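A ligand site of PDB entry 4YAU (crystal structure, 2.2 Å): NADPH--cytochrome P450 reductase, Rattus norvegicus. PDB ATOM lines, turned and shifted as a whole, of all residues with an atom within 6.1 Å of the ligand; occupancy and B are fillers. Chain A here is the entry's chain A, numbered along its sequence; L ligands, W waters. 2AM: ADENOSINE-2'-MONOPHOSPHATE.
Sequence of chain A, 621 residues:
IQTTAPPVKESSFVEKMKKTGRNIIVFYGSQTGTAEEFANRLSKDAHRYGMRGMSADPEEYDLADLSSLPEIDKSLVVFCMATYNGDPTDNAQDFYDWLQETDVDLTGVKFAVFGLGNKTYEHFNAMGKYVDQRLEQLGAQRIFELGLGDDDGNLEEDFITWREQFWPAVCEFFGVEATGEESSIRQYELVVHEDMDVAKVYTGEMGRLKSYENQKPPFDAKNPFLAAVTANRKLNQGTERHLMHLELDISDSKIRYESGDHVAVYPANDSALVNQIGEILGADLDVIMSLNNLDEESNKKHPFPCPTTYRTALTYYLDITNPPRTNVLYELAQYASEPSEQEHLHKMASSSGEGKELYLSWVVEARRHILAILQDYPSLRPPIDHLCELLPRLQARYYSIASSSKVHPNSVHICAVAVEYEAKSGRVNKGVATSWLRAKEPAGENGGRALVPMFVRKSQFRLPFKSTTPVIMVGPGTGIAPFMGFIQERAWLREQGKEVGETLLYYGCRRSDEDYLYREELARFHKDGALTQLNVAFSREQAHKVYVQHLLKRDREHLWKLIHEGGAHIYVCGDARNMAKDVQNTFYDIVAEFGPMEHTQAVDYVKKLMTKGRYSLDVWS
The side-chain amide nitrogen (NE2) of Gln 549 lies within hydrogen-bond range of a nitrogen (N1) of the ligand (3.0 Å). O of Cys 509 lies close to O3' of the ligand (3.2 Å). The side-chain carboxylate (OD2) of Asp 582 sits at hydrogen-bond distance from a nitrogen (N6) of the ligand (3.2 Å). O3P of the ligand lies within salt-bridge range of NE of Arg 540. O3P of the ligand is in salt-bridge range of NZ of Lys 545 (2.9 Å). OH of Tyr 547 is in hydrogen-bond range of O1P of the ligand (2.6 Å). An oxygen (O3') of the ligand lies within hydrogen-bond range of the side-chain hydroxyl (OG) of Ser 539, 2.7 Å away. The backbone NH (N) of Arg 510 lies within hydrogen-bond range of an oxygen (O3') of the ligand, at 3.4 Å.
SG of Cys 509 sits close to OD1 of Asp 515 (3.4 Å). The backbone NH (N) of Ser 539 is in hydrogen-bond range of the backbone carbonyl oxygen (O) of Arg 510 (3.5 Å). The backbone NH (N) of Gly 477 sits at hydrogen-bond distance from the backbone carbonyl oxygen (O) of Gly 508. The backbone NH of Asn 578 sits at hydrogen-bond distance from the side-chain carboxylate of Asp 575 (2.9 Å). The backbone NH of Ser 539 lies within hydrogen-bond range of the backbone carbonyl oxygen of Cys 509 (2.9 Å). The backbone NH (N) of Arg 510 sits at hydrogen-bond distance from the side-chain carboxylate (OD1) of Asp 515, 3.0 Å away. The backbone carbonyl oxygen of Ala 537 sits at hydrogen-bond distance from the backbone NH of Cys 509 (3.1 Å). N of Arg 540 is in hydrogen-bond range of O of Arg 510 (2.9 Å).
Residues that only touch the ligand: Pro 476 (3.9 Å), Gly 477 (3.6 Å), Gly 508 (3.97 Å), Asn 578 (3.8 Å) and Met 579 (3.5 Å). Hydrophobic or aromatic side chains within 4 Å of the ligand: Pro 476, Tyr 547 and Met 579. Within 4 Å of the ligand: Pro 476, Gly 477, Gly 508, Cys 509, Arg 510, Ser 539, Arg 540, Lys 545, Tyr 547, Gln 549, Asn 578, Met 579 and Asp 582.
Water W5 bridges a nitrogen (N3) of the ligand and the backbone NH of Val 548. Water W8 bridges the guanidinium group of Arg 510 and an oxygen (O2P) of the ligand. Water W7 bridges O3' of the ligand (2.9 Å) and O of Ala 537 (3.0 Å). Water W1 lies within hydrogen-bond range of the side-chain carboxylate of Asp 515 (2.8 Å) and the guanidinium group of Arg 241 (3.1 Å).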
ATOM      1  N   ARG A 241     -12.740   0.265 -20.718  1.00  0.00           N
ATOM      2  CA  ARG A 241     -12.072  -1.033 -20.569  1.00  0.00           C
ATOM      3  C   ARG A 241     -11.966  -1.458 -19.103  1.00  0.00           C
ATOM      4  O   ARG A 241     -12.116  -0.638 -18.180  1.00  0.00           O
ATOM      5  CB  ARG A 241     -10.656  -0.962 -21.123  1.00  0.00           C
ATOM      6  CG  ARG A 241     -10.530  -0.730 -22.619  1.00  0.00           C
ATOM      7  CD  ARG A 241      -9.075  -0.442 -22.937  1.00  0.00           C
ATOM      8  NE  ARG A 241      -8.615   0.760 -22.238  1.00  0.00           N
ATOM      9  CZ  ARG A 241      -7.344   1.141 -22.160  1.00  0.00           C
ATOM     10  NH1 ARG A 241      -6.388   0.423 -22.750  1.00  0.00           N
ATOM     11  NH2 ARG A 241      -7.024   2.254 -21.508  1.00  0.00           N
ATOM     12  N   PRO A 476       4.213  -1.848 -23.382  1.00  0.00           N
ATOM     13  CA  PRO A 476       3.079  -0.939 -23.228  1.00  0.00           C
ATOM     14  C   PRO A 476       1.809  -1.716 -22.858  1.00  0.00           C
ATOM     15  O   PRO A 476       1.734  -2.927 -23.096  1.00  0.00           O
ATOM     16  CB  PRO A 476       2.988  -0.274 -24.593  1.00  0.00           C
ATOM     17  CG  PRO A 476       3.503  -1.352 -25.528  1.00  0.00           C
ATOM     18  CD  PRO A 476       4.682  -1.901 -24.778  1.00  0.00           C
ATOM     19  N   GLY A 477       0.831  -1.047 -22.259  1.00  0.00           N
ATOM     20  CA  GLY A 477      -0.398  -1.702 -21.861  1.00  0.00           C
ATOM     21  C   GLY A 477      -0.165  -2.887 -20.928  1.00  0.00           C
ATOM     22  O   GLY A 477       0.658  -2.818 -20.019  1.00  0.00           O
ATOM     23  N   THR A 478      -0.891  -3.972 -21.166  1.00  0.00           N
ATOM     24  CA  THR A 478      -0.754  -5.181 -20.365  1.00  0.00           C
ATOM     25  C   THR A 478       0.602  -5.842 -20.587  1.00  0.00           C
ATOM     26  O   THR A 478       0.943  -6.826 -19.928  1.00  0.00           O
ATOM     27  CB  THR A 478      -1.842  -6.205 -20.690  1.00  0.00           C
ATOM     28  OG1 THR A 478      -1.905  -6.377 -22.110  1.00  0.00           O
ATOM     29  CG2 THR A 478      -3.200  -5.733 -20.131  1.00  0.00           C
ATOM     30  N   GLY A 508       3.890   2.205 -21.668  1.00  0.00           N
ATOM     31  CA  GLY A 508       2.988   3.100 -22.360  1.00  0.00           C
ATOM     32  C   GLY A 508       1.517   2.818 -22.093  1.00  0.00           C
ATOM     33  O   GLY A 508       1.109   1.682 -21.887  1.00  0.00           O
ATOM     34  N   CYS A 509       0.721   3.884 -22.106  1.00  0.00           N
ATOM     35  CA  CYS A 509      -0.722   3.788 -21.913  1.00  0.00           C
ATOM     36  C   CYS A 509      -1.306   5.046 -22.550  1.00  0.00           C
ATOM     37  O   CYS A 509      -0.575   5.893 -23.043  1.00  0.00           O
ATOM     38  CB  CYS A 509      -1.069   3.704 -20.424  1.00  0.00           C
ATOM     39  SG  CYS A 509      -0.579   5.114 -19.422  1.00  0.00           S
ATOM     40  N   ARG A 510      -2.628   5.169 -22.535  1.00  0.00           N
ATOM     41  CA  ARG A 510      -3.259   6.343 -23.147  1.00  0.00           C
ATOM     42  C   ARG A 510      -3.040   7.655 -22.383  1.00  0.00           C
ATOM     43  O   ARG A 510      -2.627   8.650 -22.978  1.00  0.00           O
ATOM     44  CB  ARG A 510      -4.760   6.100 -23.308  1.00  0.00           C
ATOM     45  CG  ARG A 510      -5.089   4.841 -24.091  1.00  0.00           C
ATOM     46  CD  ARG A 510      -6.575   4.562 -24.125  1.00  0.00           C
ATOM     47  NE  ARG A 510      -6.849   3.369 -24.924  1.00  0.00           N
ATOM     48  CZ  ARG A 510      -8.058   2.881 -25.134  1.00  0.00           C
ATOM     49  NH1 ARG A 510      -9.126   3.469 -24.613  1.00  0.00           N
ATOM     50  NH2 ARG A 510      -8.207   1.783 -25.870  1.00  0.00           N
ATOM     51  N   ASP A 515      -5.218   5.181 -17.379  1.00  0.00           N
ATOM     52  CA  ASP A 515      -4.826   3.770 -17.452  1.00  0.00           C
ATOM     53  C   ASP A 515      -3.345   3.503 -17.217  1.00  0.00           C
ATOM     54  O   ASP A 515      -2.749   2.630 -17.844  1.00  0.00           O
ATOM     55  CB  ASP A 515      -5.241   3.188 -18.813  1.00  0.00           C
ATOM     56  CG  ASP A 515      -4.553   3.870 -19.989  1.00  0.00           C
ATOM     57  OD1 ASP A 515      -3.918   4.937 -19.795  1.00  0.00           O
ATOM     58  OD2 ASP A 515      -4.652   3.349 -21.120  1.00  0.00           O
ATOM     59  N   ALA A 537       5.183   6.493 -22.277  1.00  0.00           N
ATOM     60  CA  ALA A 537       4.615   7.167 -23.441  1.00  0.00           C
ATOM     61  C   ALA A 537       3.103   7.265 -23.245  1.00  0.00           C
ATOM     62  O   ALA A 537       2.418   6.233 -23.203  1.00  0.00           O
ATOM     63  CB  ALA A 537       4.935   6.382 -24.729  1.00  0.00           C
ATOM     64  N   PHE A 538       2.581   8.476 -23.069  1.00  0.00           N
ATOM     65  CA  PHE A 538       1.136   8.678 -22.931  1.00  0.00           C
ATOM     66  C   PHE A 538       0.661   8.987 -24.341  1.00  0.00           C
ATOM     67  O   PHE A 538       0.796  10.109 -24.822  1.00  0.00           O
ATOM     68  CB  PHE A 538       0.843   9.841 -21.978  1.00  0.00           C
ATOM     69  CG  PHE A 538       1.362   9.608 -20.581  1.00  0.00           C
ATOM     70  CD1 PHE A 538       0.828   8.599 -19.787  1.00  0.00           C
ATOM     71  CD2 PHE A 538       2.429  10.349 -20.092  1.00  0.00           C
ATOM     72  CE1 PHE A 538       1.357   8.324 -18.526  1.00  0.00           C
ATOM     73  CE2 PHE A 538       2.968  10.084 -18.831  1.00  0.00           C
ATOM     74  CZ  PHE A 538       2.437   9.072 -18.046  1.00  0.00           C
ATOM     75  N   SER A 539       0.132   7.969 -25.001  1.00  0.00           N
ATOM     76  CA  SER A 539      -0.293   8.083 -26.386  1.00  0.00           C
ATOM     77  C   SER A 539      -1.395   9.077 -26.732  1.00  0.00           C
ATOM     78  O   SER A 539      -1.462   9.525 -27.876  1.00  0.00           O
ATOM     79  CB  SER A 539      -0.702   6.706 -26.891  1.00  0.00           C
ATOM     80  OG  SER A 539      -1.806   6.210 -26.156  1.00  0.00           O
ATOM     81  N   ARG A 540      -2.233   9.440 -25.771  1.00  0.00           N
ATOM     82  CA  ARG A 540      -3.336  10.364 -26.073  1.00  0.00           C
ATOM     83  C   ARG A 540      -3.357  11.711 -25.382  1.00  0.00           C
ATOM     84  O   ARG A 540      -4.337  12.446 -25.486  1.00  0.00           O
ATOM     85  CB  ARG A 540      -4.659   9.641 -25.845  1.00  0.00           C
ATOM     86  CG  ARG A 540      -4.726   8.314 -26.591  1.00  0.00           C
ATOM     87  CD  ARG A 540      -6.074   7.636 -26.529  1.00  0.00           C
ATOM     88  NE  ARG A 540      -6.018   6.314 -27.162  1.00  0.00           N
ATOM     89  CZ  ARG A 540      -7.067   5.537 -27.392  1.00  0.00           C
ATOM     90  NH1 ARG A 540      -8.277   5.955 -27.045  1.00  0.00           N
ATOM     91  NH2 ARG A 540      -6.899   4.354 -27.960  1.00  0.00           N
ATOM     92  N   LYS A 545       0.545  10.706 -31.739  1.00  0.00           N
ATOM     93  CA  LYS A 545       0.615   9.495 -30.958  1.00  0.00           C
ATOM     94  C   LYS A 545       2.053   9.481 -30.425  1.00  0.00           C
ATOM     95  O   LYS A 545       2.993   9.811 -31.156  1.00  0.00           O
ATOM     96  CB  LYS A 545       0.430   8.248 -31.843  1.00  0.00           C
ATOM     97  CG  LYS A 545      -1.000   7.969 -32.309  1.00  0.00           C
ATOM     98  CD  LYS A 545      -1.942   7.757 -31.125  1.00  0.00           C
ATOM     99  CE  LYS A 545      -3.330   7.310 -31.579  1.00  0.00           C
ATOM    100  NZ  LYS A 545      -4.301   7.241 -30.450  1.00  0.00           N
ATOM    101  N   VAL A 546       2.216   9.138 -29.155  1.00  0.00           N
ATOM    102  CA  VAL A 546       3.553   9.026 -28.588  1.00  0.00           C
ATOM    103  C   VAL A 546       3.595   7.586 -28.079  1.00  0.00           C
ATOM    104  O   VAL A 546       2.853   7.224 -27.168  1.00  0.00           O
ATOM    105  CB  VAL A 546       3.816  10.009 -27.417  1.00  0.00           C
ATOM    106  CG1 VAL A 546       5.158   9.687 -26.746  1.00  0.00           C
ATOM    107  CG2 VAL A 546       3.853  11.448 -27.945  1.00  0.00           C
ATOM    108  N   TYR A 547       4.446   6.774 -28.692  1.00  0.00           N
ATOM    109  CA  TYR A 547       4.571   5.379 -28.326  1.00  0.00           C
ATOM    110  C   TYR A 547       5.943   5.055 -27.755  1.00  0.00           C
ATOM    111  O   TYR A 547       6.860   5.867 -27.818  1.00  0.00           O
ATOM    112  CB  TYR A 547       4.302   4.494 -29.553  1.00  0.00           C
ATOM    113  CG  TYR A 547       2.894   4.598 -30.129  1.00  0.00           C
ATOM    114  CD1 TYR A 547       1.766   4.710 -29.294  1.00  0.00           C
ATOM    115  CD2 TYR A 547       2.668   4.443 -31.495  1.00  0.00           C
ATOM    116  CE1 TYR A 547       0.464   4.643 -29.824  1.00  0.00           C
ATOM    117  CE2 TYR A 547       1.389   4.373 -32.029  1.00  0.00           C
ATOM    118  CZ  TYR A 547       0.291   4.464 -31.189  1.00  0.00           C
ATOM    119  OH  TYR A 547      -0.973   4.307 -31.732  1.00  0.00           O
ATOM    120  N   VAL A 548       6.084   3.861 -27.177  1.00  0.00           N
ATOM    121  CA  VAL A 548       7.348   3.446 -26.587  1.00  0.00           C
ATOM    122  C   VAL A 548       8.540   3.542 -27.547  1.00  0.00           C
ATOM    123  O   VAL A 548       9.625   3.978 -27.161  1.00  0.00           O
ATOM    124  CB  VAL A 548       7.234   2.017 -26.009  1.00  0.00           C
ATOM    125  CG1 VAL A 548       6.280   1.991 -24.802  1.00  0.00           C
ATOM    126  CG2 VAL A 548       6.743   1.048 -27.080  1.00  0.00           C
ATOM    127  N   GLN A 549       8.340   3.146 -28.805  1.00  0.00           N
ATOM    128  CA  GLN A 549       9.430   3.186 -29.767  1.00  0.00           C
ATOM    129  C   GLN A 549       9.915   4.609 -29.977  1.00  0.00           C
ATOM    130  O   GLN A 549      11.078   4.823 -30.360  1.00  0.00           O
ATOM    131  CB  GLN A 549       9.043   2.545 -31.111  1.00  0.00           C
ATOM    132  CG  GLN A 549       7.789   3.101 -31.787  1.00  0.00           C
ATOM    133  CD  GLN A 549       6.527   2.409 -31.344  1.00  0.00           C
ATOM    134  OE1 GLN A 549       6.447   1.910 -30.228  1.00  0.00           O
ATOM    135  NE2 GLN A 549       5.540   2.348 -32.229  1.00  0.00           N
ATOM    136  N   ASP A 575       1.497  -6.430 -27.257  1.00  0.00           N
ATOM    137  CA  ASP A 575       0.940  -6.525 -28.602  1.00  0.00           C
ATOM    138  C   ASP A 575       1.937  -7.003 -29.663  1.00  0.00           C
ATOM    139  O   ASP A 575       2.901  -6.305 -29.982  1.00  0.00           O
ATOM    140  CB  ASP A 575       0.364  -5.171 -29.027  1.00  0.00           C
ATOM    141  CG  ASP A 575      -0.082  -5.158 -30.472  1.00  0.00           C
ATOM    142  OD1 ASP A 575      -0.902  -6.023 -30.834  1.00  0.00           O
ATOM    143  OD2 ASP A 575       0.394  -4.293 -31.236  1.00  0.00           O
ATOM    144  N   ASN A 578       1.191  -4.915 -33.999  1.00  0.00           N
ATOM    145  CA  ASN A 578       1.970  -3.791 -34.504  1.00  0.00           C
ATOM    146  C   ASN A 578       3.074  -3.268 -33.592  1.00  0.00           C
ATOM    147  O   ASN A 578       4.132  -2.854 -34.062  1.00  0.00           O
ATOM    148  CB  ASN A 578       1.061  -2.621 -34.882  1.00  0.00           C
ATOM    149  CG  ASN A 578       0.020  -3.005 -35.908  1.00  0.00           C
ATOM    150  OD1 ASN A 578      -1.046  -3.535 -35.578  1.00  0.00           O
ATOM    151  ND2 ASN A 578       0.320  -2.747 -37.183  1.00  0.00           N
ATOM    152  N   MET A 579       2.839  -3.287 -32.277  1.00  0.00           N
ATOM    153  CA  MET A 579       3.846  -2.776 -31.358  1.00  0.00           C
ATOM    154  C   MET A 579       5.204  -3.489 -31.474  1.00  0.00           C
ATOM    155  O   MET A 579       6.231  -2.845 -31.613  1.00  0.00           O
ATOM    156  CB  MET A 579       3.335  -2.832 -29.917  1.00  0.00           C
ATOM    157  CG  MET A 579       4.267  -2.201 -28.896  1.00  0.00           C
ATOM    158  SD  MET A 579       5.676  -3.270 -28.453  1.00  0.00           S
ATOM    159  CE  MET A 579       4.792  -4.536 -27.583  1.00  0.00           C
ATOM    160  N   ALA A 580       5.192  -4.816 -31.425  1.00  0.00           N
ATOM    161  CA  ALA A 580       6.421  -5.609 -31.489  1.00  0.00           C
ATOM    162  C   ALA A 580       7.312  -5.282 -32.684  1.00  0.00           C
ATOM    163  O   ALA A 580       8.512  -5.072 -32.528  1.00  0.00           O
ATOM    164  CB  ALA A 580       6.080  -7.093 -31.478  1.00  0.00           C
ATOM    165  N   ASP A 582       7.130  -2.535 -34.696  1.00  0.00           N
ATOM    166  CA  ASP A 582       7.551  -1.144 -34.685  1.00  0.00           C
ATOM    167  C   ASP A 582       8.740  -0.977 -33.751  1.00  0.00           C
ATOM    168  O   ASP A 582       9.673  -0.226 -34.041  1.00  0.00           O
ATOM    169  CB  ASP A 582       6.411  -0.216 -34.232  1.00  0.00           C
ATOM    170  CG  ASP A 582       5.304  -0.102 -35.256  1.00  0.00           C
ATOM    171  OD1 ASP A 582       5.575  -0.304 -36.465  1.00  0.00           O
ATOM    172  OD2 ASP A 582       4.169   0.207 -34.872  1.00  0.00           O
ATOM    173  N   VAL A 583       8.716  -1.677 -32.629  1.00  0.00           N
ATOM    174  CA  VAL A 583       9.792  -1.595 -31.657  1.00  0.00           C
ATOM    175  C   VAL A 583      11.055  -2.234 -32.233  1.00  0.00           C
ATOM    176  O   VAL A 583      12.166  -1.727 -32.049  1.00  0.00           O
ATOM    177  CB  VAL A 583       9.409  -2.298 -30.348  1.00  0.00           C
ATOM    178  CG1 VAL A 583      10.643  -2.546 -29.494  1.00  0.00           C
ATOM    179  CG2 VAL A 583       8.416  -1.438 -29.576  1.00  0.00           C
HETATM  180  P   2AM L   1      -3.236   4.122 -28.604  1.00  0.00           P
HETATM  181  O1P 2AM L   1      -2.869   3.931 -30.029  1.00  0.00           O
HETATM  182  O2P 2AM L   1      -4.238   3.159 -28.101  1.00  0.00           O
HETATM  183  O3P 2AM L   1      -3.496   5.532 -28.238  1.00  0.00           O
HETATM  184  C5' 2AM L   1      -1.497   0.206 -24.678  1.00  0.00           C
HETATM  185  O5' 2AM L   1      -2.525  -0.293 -25.530  1.00  0.00           O
HETATM  186  C4' 2AM L   1      -0.731   1.332 -25.384  1.00  0.00           C
HETATM  187  O4' 2AM L   1      -0.156   0.863 -26.610  1.00  0.00           O
HETATM  188  C3' 2AM L   1      -1.684   2.467 -25.753  1.00  0.00           C
HETATM  189  O3' 2AM L   1      -1.158   3.711 -25.278  1.00  0.00           O
HETATM  190  C2' 2AM L   1      -1.658   2.446 -27.274  1.00  0.00           C
HETATM  191  O2' 2AM L   1      -1.890   3.767 -27.801  1.00  0.00           O
HETATM  192  C1' 2AM L   1      -0.231   1.986 -27.507  1.00  0.00           C
HETATM  193  N9  2AM L   1       0.019   1.569 -28.905  1.00  0.00           N
HETATM  194  C8  2AM L   1      -0.883   1.347 -29.854  1.00  0.00           C
HETATM  195  N7  2AM L   1      -0.243   0.945 -30.951  1.00  0.00           N
HETATM  196  C5  2AM L   1       1.054   0.922 -30.678  1.00  0.00           C
HETATM  197  C6  2AM L   1       2.115   0.656 -31.449  1.00  0.00           C
HETATM  198  N6  2AM L   1       1.866   0.363 -32.723  1.00  0.00           N
HETATM  199  N1  2AM L   1       3.364   0.756 -30.990  1.00  0.00           N
HETATM  200  C2  2AM L   1       3.572   1.114 -29.652  1.00  0.00           C
HETATM  201  N3  2AM L   1       2.445   1.379 -28.867  1.00  0.00           N
HETATM  202  C4  2AM L   1       1.221   1.292 -29.411  1.00  0.00           C
HETATM  203  O   HOH W   1      -3.401   1.214 -22.402  1.00  0.00           O
HETATM  204  O   HOH W   2       0.731  -1.841 -27.707  1.00  0.00           O
HETATM  205  O   HOH W   3      -5.437   1.341 -29.558  1.00  0.00           O
HETATM  206  O   HOH W   4      -1.616   0.053 -33.589  1.00  0.00           O
HETATM  207  O   HOH W   5       3.446   2.562 -26.516  1.00  0.00           O
HETATM  208  O   HOH W   6      -4.564   3.573 -32.229  1.00  0.00           O
HETATM  209  O   HOH W   7       1.673   4.404 -25.450  1.00  0.00           O
HETATM  210  O   HOH W   8      -5.272   1.704 -25.834  1.00  0.00           O
